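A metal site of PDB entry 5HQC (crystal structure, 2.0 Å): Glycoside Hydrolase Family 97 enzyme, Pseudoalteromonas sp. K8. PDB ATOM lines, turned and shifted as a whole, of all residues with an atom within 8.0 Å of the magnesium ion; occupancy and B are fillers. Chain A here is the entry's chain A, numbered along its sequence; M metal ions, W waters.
The magnesium ion is bound by water W3 (2.0 Å), O of Gly 565 (2.0 Å), OD1 of Asp 592 (2.1 Å), OD2 of Asp 566 (2.1 Å), water W1 (2.1 Å) and water W2 (2.1 Å).
The magnesium ion has six donor atoms within binding distance.
Within 4 Å of the magnesium ion: Gly 565, Asp 566 and Asp 592.
The backbone carbonyl oxygen of Ser 476 lies within hydrogen-bond range of the backbone NH of Gly 565, at 3.0 Å.
The side-chain carboxylate (OD2) of Asp 592 is in salt-bridge range of the guanidinium group (NH2) of Arg 596, at 3.2 Å.
OD2 of Asp 592 lies within hydrogen-bond range of N of Gln 594 (3.0 Å).
The side-chain hydroxyl (OG1) of Thr 591 is in hydrogen-bond range of the side-chain carboxylate (OD2) of Asp 592 (3.2 Å).
The side-chain carboxylate (OD1) of Asp 566 lies within salt-bridge range of the guanidinium group (NH2) of Arg 596 (3.997 Å).
The side-chain hydroxyl of Ser 476 sits at hydrogen-bond distance from the backbone NH of Asp 566.
OG1 of Thr 591 sits close to O of Asp 566, at 3.4 Å.
Water W1 bridges OE1 of Glu 473 and OE1 of Glu 593.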
ATOM      1  N   TRP A 143      20.453  17.931  26.300  1.00  0.00           N
ATOM      2  CA  TRP A 143      21.507  17.540  25.367  1.00  0.00           C
ATOM      3  C   TRP A 143      22.178  18.825  24.896  1.00  0.00           C
ATOM      4  O   TRP A 143      21.558  19.613  24.184  1.00  0.00           O
ATOM      5  CB  TRP A 143      20.910  16.766  24.182  1.00  0.00           C
ATOM      6  CG  TRP A 143      20.057  15.585  24.572  1.00  0.00           C
ATOM      7  CD1 TRP A 143      20.486  14.307  24.851  1.00  0.00           C
ATOM      8  CD2 TRP A 143      18.625  15.551  24.702  1.00  0.00           C
ATOM      9  NE1 TRP A 143      19.405  13.497  25.143  1.00  0.00           N
ATOM     10  CE2 TRP A 143      18.256  14.242  25.062  1.00  0.00           C
ATOM     11  CE3 TRP A 143      17.616  16.522  24.544  1.00  0.00           C
ATOM     12  CZ2 TRP A 143      16.928  13.859  25.263  1.00  0.00           C
ATOM     13  CZ3 TRP A 143      16.288  16.139  24.745  1.00  0.00           C
ATOM     14  CH2 TRP A 143      15.959  14.824  25.095  1.00  0.00           C
ATOM     15  N   THR A 159      24.905  14.489  27.387  1.00  0.00           N
ATOM     16  CA  THR A 159      23.569  14.040  27.777  1.00  0.00           C
ATOM     17  C   THR A 159      23.533  14.014  29.302  1.00  0.00           C
ATOM     18  O   THR A 159      24.201  13.178  29.924  1.00  0.00           O
ATOM     19  CB  THR A 159      23.276  12.651  27.221  1.00  0.00           C
ATOM     20  OG1 THR A 159      23.385  12.680  25.793  1.00  0.00           O
ATOM     21  CG2 THR A 159      21.853  12.191  27.601  1.00  0.00           C
ATOM     22  N   PRO A 472      29.314   7.857  17.243  1.00  0.00           N
ATOM     23  CA  PRO A 472      28.130   7.408  16.480  1.00  0.00           C
ATOM     24  C   PRO A 472      26.866   8.238  16.701  1.00  0.00           C
ATOM     25  O   PRO A 472      26.092   8.425  15.760  1.00  0.00           O
ATOM     26  CB  PRO A 472      27.943   5.969  16.956  1.00  0.00           C
ATOM     27  CG  PRO A 472      29.413   5.500  17.201  1.00  0.00           C
ATOM     28  CD  PRO A 472      30.110   6.726  17.761  1.00  0.00           C
ATOM     29  N   GLU A 473      26.640   8.745  17.917  1.00  0.00           N
ATOM     30  CA  GLU A 473      25.402   9.489  18.199  1.00  0.00           C
ATOM     31  C   GLU A 473      25.414  10.907  17.635  1.00  0.00           C
ATOM     32  O   GLU A 473      24.373  11.578  17.705  1.00  0.00           O
ATOM     33  CB  GLU A 473      25.152   9.550  19.717  1.00  0.00           C
ATOM     34  CG  GLU A 473      26.166  10.427  20.473  1.00  0.00           C
ATOM     35  CD  GLU A 473      25.905  10.477  21.975  1.00  0.00           C
ATOM     36  OE1 GLU A 473      25.007   9.744  22.482  1.00  0.00           O
ATOM     37  OE2 GLU A 473      26.600  11.263  22.655  1.00  0.00           O
ATOM     38  N   HIS A 474      26.535  11.372  17.085  1.00  0.00           N
ATOM     39  CA  HIS A 474      26.711  12.799  16.818  1.00  0.00           C
ATOM     40  C   HIS A 474      25.629  13.362  15.889  1.00  0.00           C
ATOM     41  O   HIS A 474      25.039  14.412  16.184  1.00  0.00           O
ATOM     42  CB  HIS A 474      28.098  13.051  16.222  1.00  0.00           C
ATOM     43  CG  HIS A 474      28.441  14.505  16.092  1.00  0.00           C
ATOM     44  ND1 HIS A 474      28.379  15.387  17.152  1.00  0.00           N
ATOM     45  CD2 HIS A 474      28.844  15.236  15.018  1.00  0.00           C
ATOM     46  CE1 HIS A 474      28.738  16.589  16.748  1.00  0.00           C
ATOM     47  NE2 HIS A 474      29.013  16.534  15.454  1.00  0.00           N
ATOM     48  N   SER A 476      22.632  12.273  15.235  1.00  0.00           N
ATOM     49  CA  SER A 476      21.336  12.262  15.892  1.00  0.00           C
ATOM     50  C   SER A 476      21.252  13.286  17.010  1.00  0.00           C
ATOM     51  O   SER A 476      20.150  13.571  17.488  1.00  0.00           O
ATOM     52  CB  SER A 476      21.024  10.866  16.419  1.00  0.00           C
ATOM     53  OG  SER A 476      21.898  10.530  17.477  1.00  0.00           O
ATOM     54  N   MET A 477      22.400  13.818  17.447  1.00  0.00           N
ATOM     55  CA  MET A 477      22.416  14.964  18.357  1.00  0.00           C
ATOM     56  C   MET A 477      22.240  16.266  17.582  1.00  0.00           C
ATOM     57  O   MET A 477      21.387  17.091  17.918  1.00  0.00           O
ATOM     58  CB  MET A 477      23.726  14.985  19.151  1.00  0.00           C
ATOM     59  CG  MET A 477      23.876  13.895  20.197  1.00  0.00           C
ATOM     60  SD  MET A 477      22.697  14.143  21.544  1.00  0.00           S
ATOM     61  CE  MET A 477      23.169  12.781  22.609  1.00  0.00           C
ATOM     62  N   ALA A 563      14.423  10.553  17.828  1.00  0.00           N
ATOM     63  CA  ALA A 563      14.604  10.820  19.242  1.00  0.00           C
ATOM     64  C   ALA A 563      16.007  11.378  19.431  1.00  0.00           C
ATOM     65  O   ALA A 563      16.961  10.899  18.805  1.00  0.00           O
ATOM     66  CB  ALA A 563      14.379   9.558  20.088  1.00  0.00           C
ATOM     67  N   VAL A 564      16.127  12.392  20.284  1.00  0.00           N
ATOM     68  CA  VAL A 564      17.388  13.111  20.402  1.00  0.00           C
ATOM     69  C   VAL A 564      18.504  12.162  20.830  1.00  0.00           C
ATOM     70  O   VAL A 564      18.371  11.438  21.830  1.00  0.00           O
ATOM     71  CB  VAL A 564      17.277  14.284  21.388  1.00  0.00           C
ATOM     72  CG1 VAL A 564      18.572  15.101  21.356  1.00  0.00           C
ATOM     73  CG2 VAL A 564      16.022  15.160  21.116  1.00  0.00           C
ATOM     74  N   GLY A 565      19.610  12.167  20.093  1.00  0.00           N
ATOM     75  CA  GLY A 565      20.736  11.304  20.419  1.00  0.00           C
ATOM     76  C   GLY A 565      20.555   9.833  20.115  1.00  0.00           C
ATOM     77  O   GLY A 565      21.405   9.024  20.504  1.00  0.00           O
ATOM     78  N   ASP A 566      19.477   9.470  19.414  1.00  0.00           N
ATOM     79  CA  ASP A 566      19.199   8.083  19.042  1.00  0.00           C
ATOM     80  C   ASP A 566      19.020   7.914  17.530  1.00  0.00           C
ATOM     81  O   ASP A 566      19.708   7.077  16.943  1.00  0.00           O
ATOM     82  CB  ASP A 566      17.961   7.544  19.771  1.00  0.00           C
ATOM     83  CG  ASP A 566      18.205   7.346  21.262  1.00  0.00           C
ATOM     84  OD1 ASP A 566      17.221   7.165  22.016  1.00  0.00           O
ATOM     85  OD2 ASP A 566      19.372   7.388  21.700  1.00  0.00           O
ATOM     86  N   PHE A 567      18.095   8.638  16.892  1.00  0.00           N
ATOM     87  CA  PHE A 567      17.865   8.486  15.451  1.00  0.00           C
ATOM     88  C   PHE A 567      17.023   9.641  14.921  1.00  0.00           C
ATOM     89  O   PHE A 567      16.406  10.390  15.681  1.00  0.00           O
ATOM     90  CB  PHE A 567      17.199   7.135  15.132  1.00  0.00           C
ATOM     91  CG  PHE A 567      15.735   7.063  15.485  1.00  0.00           C
ATOM     92  CD1 PHE A 567      15.327   6.885  16.807  1.00  0.00           C
ATOM     93  CD2 PHE A 567      14.761   7.167  14.496  1.00  0.00           C
ATOM     94  CE1 PHE A 567      13.977   6.816  17.135  1.00  0.00           C
ATOM     95  CE2 PHE A 567      13.414   7.096  14.810  1.00  0.00           C
ATOM     96  CZ  PHE A 567      13.016   6.925  16.126  1.00  0.00           C
ATOM     97  N   THR A 591      21.102   6.348  12.654  1.00  0.00           N
ATOM     98  CA  THR A 591      20.988   5.959  14.052  1.00  0.00           C
ATOM     99  C   THR A 591      22.257   6.365  14.796  1.00  0.00           C
ATOM    100  O   THR A 591      23.184   6.941  14.205  1.00  0.00           O
ATOM    101  CB  THR A 591      20.728   4.454  14.186  1.00  0.00           C
ATOM    102  OG1 THR A 591      20.499   4.118  15.561  1.00  0.00           O
ATOM    103  CG2 THR A 591      21.937   3.668  13.640  1.00  0.00           C
ATOM    104  N   ASP A 592      22.296   6.054  16.086  1.00  0.00           N
ATOM    105  CA  ASP A 592      23.452   6.314  16.933  1.00  0.00           C
ATOM    106  C   ASP A 592      24.332   5.055  17.019  1.00  0.00           C
ATOM    107  O   ASP A 592      24.470   4.335  16.023  1.00  0.00           O
ATOM    108  CB  ASP A 592      22.989   6.763  18.333  1.00  0.00           C
ATOM    109  CG  ASP A 592      22.065   5.751  19.008  1.00  0.00           C
ATOM    110  OD1 ASP A 592      21.547   6.026  20.121  1.00  0.00           O
ATOM    111  OD2 ASP A 592      21.847   4.672  18.414  1.00  0.00           O
ATOM    112  N   GLU A 593      24.894   4.743  18.194  1.00  0.00           N
ATOM    113  CA  GLU A 593      25.734   3.550  18.286  1.00  0.00           C
ATOM    114  C   GLU A 593      24.936   2.251  18.225  1.00  0.00           C
ATOM    115  O   GLU A 593      25.538   1.185  18.048  1.00  0.00           O
ATOM    116  CB  GLU A 593      26.579   3.584  19.571  1.00  0.00           C
ATOM    117  CG  GLU A 593      25.778   3.371  20.875  1.00  0.00           C
ATOM    118  CD  GLU A 593      24.913   4.554  21.294  1.00  0.00           C
ATOM    119  OE1 GLU A 593      25.073   5.682  20.751  1.00  0.00           O
ATOM    120  OE2 GLU A 593      24.069   4.364  22.190  1.00  0.00           O
ATOM    121  N   GLN A 594      23.607   2.294  18.352  1.00  0.00           N
ATOM    122  CA  GLN A 594      22.778   1.098  18.346  1.00  0.00           C
ATOM    123  C   GLN A 594      22.225   0.819  16.947  1.00  0.00           C
ATOM    124  O   GLN A 594      21.757   1.733  16.260  1.00  0.00           O
ATOM    125  CB  GLN A 594      21.610   1.236  19.333  1.00  0.00           C
ATOM    126  CG  GLN A 594      22.043   1.346  20.806  1.00  0.00           C
ATOM    127  CD  GLN A 594      20.859   1.322  21.778  1.00  0.00           C
ATOM    128  OE1 GLN A 594      19.716   1.078  21.375  1.00  0.00           O
ATOM    129  NE2 GLN A 594      21.137   1.578  23.052  1.00  0.00           N
ATOM    130  N   ARG A 596      19.158  -0.268  14.792  1.00  0.00           N
ATOM    131  CA  ARG A 596      17.784   0.154  15.042  1.00  0.00           C
ATOM    132  C   ARG A 596      16.878  -0.250  13.892  1.00  0.00           C
ATOM    133  O   ARG A 596      17.247  -0.106  12.729  1.00  0.00           O
ATOM    134  CB  ARG A 596      17.669   1.679  15.238  1.00  0.00           C
ATOM    135  CG  ARG A 596      17.978   2.172  16.638  1.00  0.00           C
ATOM    136  CD  ARG A 596      17.809   3.695  16.840  1.00  0.00           C
ATOM    137  NE  ARG A 596      18.688   4.067  17.949  1.00  0.00           N
ATOM    138  CZ  ARG A 596      18.349   3.904  19.223  1.00  0.00           C
ATOM    139  NH1 ARG A 596      17.141   3.435  19.514  1.00  0.00           N
ATOM    140  NH2 ARG A 596      19.215   4.218  20.196  1.00  0.00           N
HETATM  141 MG    MG M   1      21.463   7.382  21.669  1.00  0.00          MG
HETATM  142  O   HOH W   1      23.526   7.606  21.964  1.00  0.00           O
HETATM  143  O   HOH W   2      21.382   8.685  23.355  1.00  0.00           O
HETATM  144  O   HOH W   3      21.648   5.791  22.797  1.00  0.00           O
